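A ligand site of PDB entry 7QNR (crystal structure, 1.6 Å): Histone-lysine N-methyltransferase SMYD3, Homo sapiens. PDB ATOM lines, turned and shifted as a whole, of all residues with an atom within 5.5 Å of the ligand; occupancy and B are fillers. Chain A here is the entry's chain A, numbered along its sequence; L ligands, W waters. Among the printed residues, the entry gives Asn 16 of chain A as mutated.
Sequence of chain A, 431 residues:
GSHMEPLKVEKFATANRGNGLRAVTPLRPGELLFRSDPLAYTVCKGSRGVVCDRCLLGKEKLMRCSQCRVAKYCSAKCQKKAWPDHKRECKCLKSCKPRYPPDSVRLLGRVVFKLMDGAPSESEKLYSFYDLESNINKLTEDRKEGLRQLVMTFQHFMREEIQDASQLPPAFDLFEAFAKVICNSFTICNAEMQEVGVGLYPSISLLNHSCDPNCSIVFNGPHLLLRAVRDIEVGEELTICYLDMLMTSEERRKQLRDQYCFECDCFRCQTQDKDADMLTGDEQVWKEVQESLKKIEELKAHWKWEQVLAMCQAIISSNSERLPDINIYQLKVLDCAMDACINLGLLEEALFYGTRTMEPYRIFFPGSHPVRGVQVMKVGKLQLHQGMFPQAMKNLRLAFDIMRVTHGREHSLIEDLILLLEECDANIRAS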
ATOM      1  N   ASN A  16      20.603 -13.337  -3.739  1.00  0.00           N
ATOM      2  CA  ASN A  16      21.337 -12.541  -4.713  1.00  0.00           C
ATOM      3  C   ASN A  16      20.728 -11.183  -5.044  1.00  0.00           C
ATOM      4  O   ASN A  16      21.017 -10.637  -6.111  1.00  0.00           O
ATOM      5  CB  ASN A  16      21.483 -13.330  -6.031  1.00  0.00           C
ATOM      6  CG  ASN A  16      20.149 -13.798  -6.582  1.00  0.00           C
ATOM      7  OD1 ASN A  16      19.145 -13.076  -6.510  1.00  0.00           O
ATOM      8  ND2 ASN A  16      20.125 -14.987  -7.148  1.00  0.00           N
ATOM      9  N   ARG A  17      19.890 -10.618  -4.184  1.00  0.00           N
ATOM     10  CA  ARG A  17      19.312  -9.292  -4.421  1.00  0.00           C
ATOM     11  C   ARG A  17      19.171  -8.530  -3.120  1.00  0.00           C
ATOM     12  O   ARG A  17      18.157  -7.880  -2.858  1.00  0.00           O
ATOM     13  CB  ARG A  17      17.971  -9.390  -5.154  1.00  0.00           C
ATOM     14  CG  ARG A  17      17.060 -10.517  -4.738  1.00  0.00           C
ATOM     15  CD  ARG A  17      16.160 -10.964  -5.900  1.00  0.00           C
ATOM     16  NE  ARG A  17      16.950 -11.369  -7.065  1.00  0.00           N
ATOM     17  CZ  ARG A  17      16.439 -11.730  -8.234  1.00  0.00           C
ATOM     18  NH1 ARG A  17      17.215 -12.073  -9.246  1.00  0.00           N
ATOM     19  NH2 ARG A  17      15.121 -11.742  -8.386  1.00  0.00           N
ATOM     20  N   GLY A  18      20.203  -8.590  -2.275  1.00  0.00           N
ATOM     21  CA  GLY A  18      20.213  -7.846  -1.053  1.00  0.00           C
ATOM     22  C   GLY A  18      19.119  -8.301  -0.103  1.00  0.00           C
ATOM     23  O   GLY A  18      18.756  -9.471  -0.026  1.00  0.00           O
ATOM     24  N   ASN A  19      18.576  -7.337   0.637  1.00  0.00           N
ATOM     25  CA  ASN A  19      17.478  -7.636   1.545  1.00  0.00           C
ATOM     26  C   ASN A  19      16.171  -7.652   0.790  1.00  0.00           C
ATOM     27  O   ASN A  19      16.022  -7.000  -0.258  1.00  0.00           O
ATOM     28  CB  ASN A  19      17.407  -6.640   2.694  1.00  0.00           C
ATOM     29  CG  ASN A  19      18.647  -6.704   3.573  1.00  0.00           C
ATOM     30  OD1 ASN A  19      19.025  -7.774   4.041  1.00  0.00           O
ATOM     31  ND2 ASN A  19      19.263  -5.560   3.787  1.00  0.00           N
ATOM     32  N   GLY A  20      15.218  -8.397   1.316  1.00  0.00           N
ATOM     33  CA  GLY A  20      13.898  -8.465   0.712  1.00  0.00           C
ATOM     34  C   GLY A  20      12.826  -8.613   1.765  1.00  0.00           C
ATOM     35  O   GLY A  20      13.119  -8.549   2.973  1.00  0.00           O
ATOM     36  N   TYR A 127      12.706  -1.054   8.252  1.00  0.00           N
ATOM     37  CA  TYR A 127      13.859  -0.719   7.419  1.00  0.00           C
ATOM     38  C   TYR A 127      13.935   0.807   7.402  1.00  0.00           C
ATOM     39  O   TYR A 127      12.906   1.458   7.225  1.00  0.00           O
ATOM     40  CB  TYR A 127      13.675  -1.333   6.047  1.00  0.00           C
ATOM     41  CG  TYR A 127      14.927  -1.652   5.241  1.00  0.00           C
ATOM     42  CD1 TYR A 127      15.872  -2.546   5.723  1.00  0.00           C
ATOM     43  CD2 TYR A 127      15.089  -1.152   3.963  1.00  0.00           C
ATOM     44  CE1 TYR A 127      16.986  -2.872   4.980  1.00  0.00           C
ATOM     45  CE2 TYR A 127      16.189  -1.483   3.194  1.00  0.00           C
ATOM     46  CZ  TYR A 127      17.136  -2.334   3.711  1.00  0.00           C
ATOM     47  OH  TYR A 127      18.243  -2.689   2.958  1.00  0.00           O
ATOM     48  N   ASP A 131      19.282   2.323   6.265  1.00  0.00           N
ATOM     49  CA  ASP A 131      19.474   0.970   5.753  1.00  0.00           C
ATOM     50  C   ASP A 131      19.381   0.876   4.250  1.00  0.00           C
ATOM     51  O   ASP A 131      19.760  -0.161   3.698  1.00  0.00           O
ATOM     52  CB  ASP A 131      18.415   0.029   6.359  1.00  0.00           C
ATOM     53  CG  ASP A 131      18.525  -0.102   7.854  1.00  0.00           C
ATOM     54  OD1 ASP A 131      19.660  -0.204   8.380  1.00  0.00           O
ATOM     55  OD2 ASP A 131      17.454  -0.116   8.520  1.00  0.00           O
ATOM     56  N   LEU A 132      18.869   1.902   3.560  1.00  0.00           N
ATOM     57  CA  LEU A 132      18.484   1.764   2.173  1.00  0.00           C
ATOM     58  C   LEU A 132      19.692   1.485   1.284  1.00  0.00           C
ATOM     59  O   LEU A 132      20.787   2.007   1.521  1.00  0.00           O
ATOM     60  CB  LEU A 132      17.781   3.024   1.677  1.00  0.00           C
ATOM     61  CG  LEU A 132      16.459   3.365   2.379  1.00  0.00           C
ATOM     62  CD1 LEU A 132      15.956   4.710   1.898  1.00  0.00           C
ATOM     63  CD2 LEU A 132      15.431   2.282   2.124  1.00  0.00           C
ATOM     64  N   GLU A 133      19.466   0.661   0.257  1.00  0.00           N
ATOM     65  CA  GLU A 133      20.458   0.380  -0.765  1.00  0.00           C
ATOM     66  C   GLU A 133      20.838   1.640  -1.524  1.00  0.00           C
ATOM     67  O   GLU A 133      19.976   2.433  -1.911  1.00  0.00           O
ATOM     68  CB  GLU A 133      19.878  -0.638  -1.754  1.00  0.00           C
ATOM     69  CG  GLU A 133      20.796  -1.018  -2.894  1.00  0.00           C
ATOM     70  CD  GLU A 133      22.046  -1.711  -2.416  1.00  0.00           C
ATOM     71  OE1 GLU A 133      21.937  -2.887  -2.009  1.00  0.00           O
ATOM     72  OE2 GLU A 133      23.129  -1.084  -2.459  1.00  0.00           O
ATOM     73  N   ASN A 135      23.698   1.223  -3.974  1.00  0.00           N
ATOM     74  CA  ASN A 135      24.260   0.674  -5.208  1.00  0.00           C
ATOM     75  C   ASN A 135      25.477   1.478  -5.681  1.00  0.00           C
ATOM     76  O   ASN A 135      25.803   1.477  -6.864  1.00  0.00           O
ATOM     77  CB  ASN A 135      23.221   0.611  -6.333  1.00  0.00           C
ATOM     78  CG  ASN A 135      22.253  -0.518  -6.163  1.00  0.00           C
ATOM     79  OD1 ASN A 135      22.638  -1.639  -5.814  1.00  0.00           O
ATOM     80  ND2 ASN A 135      20.977  -0.246  -6.395  1.00  0.00           N
ATOM     81  N   LYS A 138      28.008   0.129  -8.042  1.00  0.00           N
ATOM     82  CA  LYS A 138      27.547  -0.169  -9.396  1.00  0.00           C
ATOM     83  C   LYS A 138      27.277   1.079 -10.225  1.00  0.00           C
ATOM     84  O   LYS A 138      27.037   0.958 -11.437  1.00  0.00           O
ATOM     85  CB  LYS A 138      26.284  -1.038  -9.354  1.00  0.00           C
ATOM     86  CG  LYS A 138      26.533  -2.472  -8.964  1.00  0.00           C
ATOM     87  CD  LYS A 138      25.222  -3.222  -8.761  1.00  0.00           C
ATOM     88  CE  LYS A 138      25.455  -4.708  -8.570  1.00  0.00           C
ATOM     89  NZ  LYS A 138      24.178  -5.454  -8.295  1.00  0.00           N
ATOM     90  N   CYS A 183      17.218   5.004  -6.177  1.00  0.00           N
ATOM     91  CA  CYS A 183      16.677   3.653  -6.296  1.00  0.00           C
ATOM     92  C   CYS A 183      15.684   3.286  -5.214  1.00  0.00           C
ATOM     93  O   CYS A 183      15.322   2.115  -5.095  1.00  0.00           O
ATOM     94  CB  CYS A 183      17.805   2.623  -6.301  1.00  0.00           C
ATOM     95  SG  CYS A 183      18.842   2.722  -4.848  1.00  0.00           S
ATOM     96  N   ASN A 184      15.211   4.272  -4.421  1.00  0.00           N
ATOM     97  CA  ASN A 184      14.210   4.002  -3.398  1.00  0.00           C
ATOM     98  C   ASN A 184      13.091   5.033  -3.391  1.00  0.00           C
ATOM     99  O   ASN A 184      12.339   5.118  -2.415  1.00  0.00           O
ATOM    100  CB  ASN A 184      14.857   3.945  -2.020  1.00  0.00           C
ATOM    101  CG  ASN A 184      15.821   2.779  -1.877  1.00  0.00           C
ATOM    102  OD1 ASN A 184      15.405   1.630  -1.699  1.00  0.00           O
ATOM    103  ND2 ASN A 184      17.101   3.078  -1.992  1.00  0.00           N
ATOM    104  N   SER A 205      10.511  -0.097   0.867  1.00  0.00           N
ATOM    105  CA  SER A 205      11.679  -0.264   0.012  1.00  0.00           C
ATOM    106  C   SER A 205      12.345  -1.615   0.176  1.00  0.00           C
ATOM    107  O   SER A 205      13.261  -1.928  -0.595  1.00  0.00           O
ATOM    108  CB  SER A 205      12.703   0.845   0.284  1.00  0.00           C
ATOM    109  OG  SER A 205      12.262   2.071  -0.281  1.00  0.00           O
ATOM    110  N   LEU A 206      11.914  -2.432   1.125  1.00  0.00           N
ATOM    111  CA  LEU A 206      12.418  -3.802   1.195  1.00  0.00           C
ATOM    112  C   LEU A 206      11.938  -4.648   0.022  1.00  0.00           C
ATOM    113  O   LEU A 206      12.534  -5.688  -0.261  1.00  0.00           O
ATOM    114  CB  LEU A 206      11.995  -4.466   2.508  1.00  0.00           C
ATOM    115  CG  LEU A 206      12.878  -4.188   3.713  1.00  0.00           C
ATOM    116  CD1 LEU A 206      12.243  -4.747   4.957  1.00  0.00           C
ATOM    117  CD2 LEU A 206      14.270  -4.778   3.498  1.00  0.00           C
ATOM    118  N   LEU A 207      10.864  -4.237  -0.668  1.00  0.00           N
ATOM    119  CA  LEU A 207      10.309  -5.044  -1.740  1.00  0.00           C
ATOM    120  C   LEU A 207      11.207  -4.998  -2.966  1.00  0.00           C
ATOM    121  O   LEU A 207      11.491  -3.917  -3.510  1.00  0.00           O
ATOM    122  CB  LEU A 207       8.915  -4.548  -2.104  1.00  0.00           C
ATOM    123  CG  LEU A 207       7.830  -4.733  -1.033  1.00  0.00           C
ATOM    124  CD1 LEU A 207       6.723  -3.744  -1.258  1.00  0.00           C
ATOM    125  CD2 LEU A 207       7.326  -6.162  -1.081  1.00  0.00           C
ATOM    126  N   ASN A 208      11.657  -6.162  -3.411  1.00  0.00           N
ATOM    127  CA  ASN A 208      12.388  -6.249  -4.658  1.00  0.00           C
ATOM    128  C   ASN A 208      11.410  -6.240  -5.834  1.00  0.00           C
ATOM    129  O   ASN A 208      10.184  -6.301  -5.661  1.00  0.00           O
ATOM    130  CB  ASN A 208      13.258  -7.491  -4.683  1.00  0.00           C
ATOM    131  CG  ASN A 208      14.508  -7.331  -3.824  1.00  0.00           C
ATOM    132  OD1 ASN A 208      15.203  -6.319  -3.906  1.00  0.00           O
ATOM    133  ND2 ASN A 208      14.796  -8.326  -3.004  1.00  0.00           N
ATOM    134  N   HIS A 209      11.972  -6.136  -7.031  1.00  0.00           N
ATOM    135  CA  HIS A 209      11.217  -5.951  -8.258  1.00  0.00           C
ATOM    136  C   HIS A 209      10.958  -7.280  -8.957  1.00  0.00           C
ATOM    137  O   HIS A 209      11.788  -8.199  -8.964  1.00  0.00           O
ATOM    138  CB  HIS A 209      11.978  -5.041  -9.225  1.00  0.00           C
ATOM    139  CG  HIS A 209      11.450  -5.073 -10.623  1.00  0.00           C
ATOM    140  ND1 HIS A 209      10.397  -4.292 -11.023  1.00  0.00           N
ATOM    141  CD2 HIS A 209      11.785  -5.831 -11.690  1.00  0.00           C
ATOM    142  CE1 HIS A 209      10.121  -4.546 -12.292  1.00  0.00           C
ATOM    143  NE2 HIS A 209      10.942  -5.478 -12.718  1.00  0.00           N
ATOM    144  N   SER A 210       9.790  -7.358  -9.594  1.00  0.00           N
ATOM    145  CA  SER A 210       9.495  -8.388 -10.567  1.00  0.00           C
ATOM    146  C   SER A 210       8.626  -7.775 -11.644  1.00  0.00           C
ATOM    147  O   SER A 210       7.745  -6.959 -11.349  1.00  0.00           O
ATOM    148  CB  SER A 210       8.785  -9.598  -9.940  1.00  0.00           C
ATOM    149  OG  SER A 210       8.474 -10.548 -10.946  1.00  0.00           O
ATOM    150  N   TYR A 242       8.428  -2.219 -10.236  1.00  0.00           N
ATOM    151  CA  TYR A 242       8.879  -0.841 -10.129  1.00  0.00           C
ATOM    152  C   TYR A 242       8.442   0.003 -11.322  1.00  0.00           C
ATOM    153  O   TYR A 242       8.564   1.227 -11.245  1.00  0.00           O
ATOM    154  CB  TYR A 242      10.415  -0.765 -10.038  1.00  0.00           C
ATOM    155  CG  TYR A 242      11.071  -1.407  -8.836  1.00  0.00           C
ATOM    156  CD1 TYR A 242      10.325  -1.995  -7.827  1.00  0.00           C
ATOM    157  CD2 TYR A 242      12.458  -1.403  -8.713  1.00  0.00           C
ATOM    158  CE1 TYR A 242      10.941  -2.583  -6.724  1.00  0.00           C
ATOM    159  CE2 TYR A 242      13.074  -1.959  -7.612  1.00  0.00           C
ATOM    160  CZ  TYR A 242      12.322  -2.532  -6.622  1.00  0.00           C
ATOM    161  OH  TYR A 242      12.944  -3.091  -5.551  1.00  0.00           O
ATOM    162  N   GLN A 259      18.501   3.032 -13.458  1.00  0.00           N
ATOM    163  CA  GLN A 259      18.012   3.556 -12.183  1.00  0.00           C
ATOM    164  C   GLN A 259      18.261   2.620 -11.014  1.00  0.00           C
ATOM    165  O   GLN A 259      18.548   3.094  -9.904  1.00  0.00           O
ATOM    166  CB  GLN A 259      16.515   3.851 -12.297  1.00  0.00           C
ATOM    167  CG  GLN A 259      15.944   4.476 -11.033  1.00  0.00           C
ATOM    168  CD  GLN A 259      14.484   4.846 -11.181  1.00  0.00           C
ATOM    169  OE1 GLN A 259      13.874   4.645 -12.242  1.00  0.00           O
ATOM    170  NE2 GLN A 259      13.900   5.379 -10.126  1.00  0.00           N
ATOM    171  N   TYR A 260      18.180   1.309 -11.224  1.00  0.00           N
ATOM    172  CA  TYR A 260      18.209   0.353 -10.119  1.00  0.00           C
ATOM    173  C   TYR A 260      19.421  -0.552 -10.144  1.00  0.00           C
ATOM    174  O   TYR A 260      19.590  -1.356  -9.221  1.00  0.00           O
ATOM    175  CB  TYR A 260      16.934  -0.487 -10.115  1.00  0.00           C
ATOM    176  CG  TYR A 260      15.686   0.359  -9.880  1.00  0.00           C
ATOM    177  CD1 TYR A 260      15.373   0.814  -8.608  1.00  0.00           C
ATOM    178  CD2 TYR A 260      14.867   0.708 -10.925  1.00  0.00           C
ATOM    179  CE1 TYR A 260      14.251   1.587  -8.377  1.00  0.00           C
ATOM    180  CE2 TYR A 260      13.733   1.500 -10.692  1.00  0.00           C
ATOM    181  CZ  TYR A 260      13.442   1.927  -9.423  1.00  0.00           C
ATOM    182  OH  TYR A 260      12.340   2.691  -9.190  1.00  0.00           O
ATOM    183  N   CYS A 261      20.272  -0.451 -11.163  1.00  0.00           N
ATOM    184  CA  CYS A 261      21.543  -1.162 -11.195  1.00  0.00           C
ATOM    185  C   CYS A 261      21.374  -2.681 -11.037  1.00  0.00           C
ATOM    186  O   CYS A 261      22.096  -3.327 -10.267  1.00  0.00           O
ATOM    187  CB  CYS A 261      22.490  -0.618 -10.112  1.00  0.00           C
ATOM    188  SG  CYS A 261      23.065   1.039 -10.356  1.00  0.00           S
ATOM    189  N   PHE A 262      20.421  -3.257 -11.769  1.00  0.00           N
ATOM    190  CA  PHE A 262      20.377  -4.713 -11.810  1.00  0.00           C
ATOM    191  C   PHE A 262      19.844  -5.188 -13.144  1.00  0.00           C
ATOM    192  O   PHE A 262      19.186  -4.438 -13.892  1.00  0.00           O
ATOM    193  CB  PHE A 262      19.573  -5.299 -10.632  1.00  0.00           C
ATOM    194  CG  PHE A 262      18.070  -5.136 -10.753  1.00  0.00           C
ATOM    195  CD1 PHE A 262      17.446  -4.032 -10.214  1.00  0.00           C
ATOM    196  CD2 PHE A 262      17.302  -6.115 -11.358  1.00  0.00           C
ATOM    197  CE1 PHE A 262      16.073  -3.874 -10.319  1.00  0.00           C
ATOM    198  CE2 PHE A 262      15.926  -5.960 -11.453  1.00  0.00           C
ATOM    199  CZ  PHE A 262      15.316  -4.850 -10.931  1.00  0.00           C
ATOM    200  N   GLU A 263      20.182  -6.440 -13.447  1.00  0.00           N
ATOM    201  CA  GLU A 263      19.815  -7.105 -14.683  1.00  0.00           C
ATOM    202  C   GLU A 263      18.659  -8.026 -14.335  1.00  0.00           C
ATOM    203  O   GLU A 263      18.829  -8.961 -13.544  1.00  0.00           O
ATOM    204  CB  GLU A 263      20.988  -7.914 -15.231  1.00  0.00           C
ATOM    205  CG  GLU A 263      22.335  -7.175 -15.227  1.00  0.00           C
ATOM    206  CD  GLU A 263      22.352  -5.963 -16.143  1.00  0.00           C
ATOM    207  OE1 GLU A 263      21.414  -5.831 -16.958  1.00  0.00           O
ATOM    208  OE2 GLU A 263      23.312  -5.150 -16.065  1.00  0.00           O
ATOM    209  N   CYS A 264      17.485  -7.754 -14.885  1.00  0.00           N
ATOM    210  CA  CYS A 264      16.300  -8.529 -14.513  1.00  0.00           C
ATOM    211  C   CYS A 264      16.343  -9.895 -15.179  1.00  0.00           C
ATOM    212  O   CYS A 264      16.472 -10.006 -16.393  1.00  0.00           O
ATOM    213  CB  CYS A 264      15.016  -7.805 -14.884  1.00  0.00           C
ATOM    214  SG  CYS A 264      13.617  -8.738 -14.178  1.00  0.00           S
ATOM    215  N   ASP A 265      16.201 -10.944 -14.361  1.00  0.00           N
ATOM    216  CA  ASP A 265      16.246 -12.326 -14.807  1.00  0.00           C
ATOM    217  C   ASP A 265      14.881 -12.991 -14.783  1.00  0.00           C
ATOM    218  O   ASP A 265      14.796 -14.213 -14.937  1.00  0.00           O
ATOM    219  CB  ASP A 265      17.236 -13.114 -13.935  1.00  0.00           C
ATOM    220  CG  ASP A 265      16.757 -13.263 -12.509  1.00  0.00           C
ATOM    221  OD1 ASP A 265      15.783 -12.574 -12.111  1.00  0.00           O
ATOM    222  OD2 ASP A 265      17.360 -14.053 -11.742  1.00  0.00           O
HETATM  223  N1  LIG L   1      17.246  -5.278  -2.221  1.00  0.00           N
HETATM  224  C1  LIG L   1      16.998  -3.947  -1.684  1.00  0.00           C
HETATM  225  C2  LIG L   1      17.730  -3.758  -0.346  1.00  0.00           C
HETATM  226  O1  LIG L   1      17.540  -2.748   0.325  1.00  0.00           O
HETATM  227  O2  LIG L   1      18.522  -4.609   0.084  1.00  0.00           O
HETATM  228  C3  LIG L   1      15.497  -3.698  -1.505  1.00  0.00           C
HETATM  229  C4  LIG L   1      14.828  -3.183  -2.778  1.00  0.00           C
HETATM  230  S1  LIG L   1      15.382  -1.502  -3.157  1.00  0.00           S
HETATM  231  C5  LIG L   1      13.801  -0.629  -3.359  1.00  0.00           C
HETATM  232  C6  LIG L   1      15.816  -1.643  -4.908  1.00  0.00           C
HETATM  233  C7  LIG L   1      17.168  -2.278  -5.124  1.00  0.00           C
HETATM  234  O3  LIG L   1      17.138  -3.680  -4.818  1.00  0.00           O
HETATM  235  C8  LIG L   1      17.675  -2.150  -6.581  1.00  0.00           C
HETATM  236  O4  LIG L   1      18.389  -0.994  -6.809  1.00  0.00           O
HETATM  237  C9  LIG L   1      18.540  -3.414  -6.721  1.00  0.00           C
HETATM  238  O5  LIG L   1      19.814  -3.139  -6.206  1.00  0.00           O
HETATM  239  C10 LIG L   1      17.830  -4.423  -5.834  1.00  0.00           C
HETATM  240  N2  LIG L   1      16.842  -5.218  -6.572  1.00  0.00           N
HETATM  241  C11 LIG L   1      15.479  -4.989  -6.591  1.00  0.00           C
HETATM  242  N3  LIG L   1      14.905  -5.923  -7.385  1.00  0.00           N
HETATM  243  C12 LIG L   1      15.869  -6.746  -7.866  1.00  0.00           C
HETATM  244  C13 LIG L   1      15.831  -7.855  -8.699  1.00  0.00           C
HETATM  245  N4  LIG L   1      14.680  -8.312  -9.196  1.00  0.00           N
HETATM  246  N5  LIG L   1      17.002  -8.497  -9.020  1.00  0.00           N
HETATM  247  C14 LIG L   1      18.199  -8.042  -8.503  1.00  0.00           C
HETATM  248  N6  LIG L   1      18.231  -6.949  -7.686  1.00  0.00           N
HETATM  249  C15 LIG L   1      17.087  -6.300  -7.347  1.00  0.00           C
HETATM  250  O   HOH W   1      19.934  -4.910  -3.232  1.00  0.00           O
HETATM  251  O   HOH W   2      14.228 -10.353 -11.446  1.00  0.00           O
HETATM  252  O   HOH W   3      21.875  -3.935  -7.705  1.00  0.00           O
HETATM  253  O   HOH W   4      20.985  -6.685  -7.236  1.00  0.00           O
HETATM  254  O   HOH W   5      17.353 -10.233 -11.317  1.00  0.00           O
HETATM  255  O   HOH W   6      21.178  -3.936   0.799  1.00  0.00           O
HETATM  256  O   HOH W   7      10.493  -1.223  -3.089  1.00  0.00           O
HETATM  257  O   HOH W   8      16.799  -0.187  -0.117  1.00  0.00           O
HETATM  258  O   HOH W   9      11.291   1.594  -3.836  1.00  0.00           O
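The side-chain amide oxygen of Asn 184 lies close to a sulfur (S1) of the ligand, 3.5 Å away. The backbone carbonyl oxygen (O) of Ser 205 sits close to a sulfur (S1) of the ligand. The side-chain hydroxyl of Tyr 242 sits close to a sulfur (S1) of the ligand, 3.8 Å away. Gly 18 touches the ligand. CB of Glu 133 touches O1 of the ligand, 3.8 Å away. O of Cys 183 touches C5 of the ligand (3.6 Å). Leu 206 touches the ligand (O to C3, 3.8 Å). O of Leu 207 touches C4 of the ligand (3.5 Å). Phe 262 touches the ligand (CE2 to C13, 3.3 Å). Hydrophobic or aromatic side chains within 4 Å of the ligand: Tyr 127, His 209, Tyr 242, Tyr 260 and Phe 262. Along chain A the residues within 4 Å of the ligand span positions 17 to 262.
Water W3 lies within hydrogen-bond range of the backbone carbonyl oxygen of Cys 261 (2.6 Å), an oxygen (O5) of the ligand (2.7 Å), the side-chain amino group of Lys 138 (2.8 Å) and the side-chain amide oxygen of Asn 135 (3.1 Å). Water W8 lies within hydrogen-bond range of O1 of the ligand (2.7 Å), OD1 of Asn 184 (2.8 Å) and N of Glu 133 (2.8 Å). Water W6 lies within hydrogen-bond range of an oxygen (O2) of the ligand and the side-chain carboxylate of Glu 133. Water W1 lies within hydrogen-bond range of N1 of the ligand (2.9 Å), OE1 of Glu 133 (3.1 Å) and O of Arg 17 (3.5 Å). Water W2 lies within hydrogen-bond range of the side-chain carboxylate (OD1) of Asp 265, a nitrogen (N4) of the ligand and the guanidinium group (NH2) of Arg 17.
O of Arg 17 sits at hydrogen-bond distance from N1 of the ligand, at 2.8 Å. A nitrogen (N5) of the ligand lies close to the guanidinium group (NE) of Arg 17 (3.5 Å). The side-chain amide nitrogen (ND2) of Asn 135 sits at hydrogen-bond distance from an oxygen (O4) of the ligand, at 2.7 Å. O of Tyr 260 sits at hydrogen-bond distance from O4 of the ligand (2.7 Å). The side-chain amide oxygen (OD1) of Asn 208 is in hydrogen-bond range of a nitrogen (N1) of the ligand, at 2.8 Å. The backbone carbonyl oxygen of His 209 lies within hydrogen-bond range of a nitrogen (N4) of the ligand, at 2.9 Å. O of Asn 19 is in hydrogen-bond range of N1 of the ligand, at 2.9 Å. The backbone NH (N) of Asn 19 sits at hydrogen-bond distance from an oxygen (O2) of the ligand. OH of Tyr 127 sits at hydrogen-bond distance from O1 of the ligand (2.7 Å). N of His 209 lies within hydrogen-bond range of N3 of the ligand, at 3.0 Å.
The backbone NH (N) of Asn 135 lies within hydrogen-bond range of the side-chain carboxylate (OE2) of Glu 133. ND2 of Asn 184 lies within hydrogen-bond range of SG of Cys 183 (3.4 Å). ND2 of Asn 19 sits at hydrogen-bond distance from OH of Tyr 127, 3.2 Å away. OD2 of Asp 265 is in salt-bridge range of NH1 of Arg 17. The side-chain sulfur (SG) of Cys 183 sits at hydrogen-bond distance from the backbone carbonyl oxygen (O) of Glu 133 (3.2 Å). The side-chain amide nitrogen (ND2) of Asn 135 sits at hydrogen-bond distance from the backbone carbonyl oxygen (O) of Tyr 260 (3.3 Å). N of Tyr 242 lies within hydrogen-bond range of ND1 of His 209 (3.0 Å). The side-chain amide nitrogen (NE2) of Gln 259 is in hydrogen-bond range of the side-chain hydroxyl (OH) of Tyr 260, at 3.2 Å.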
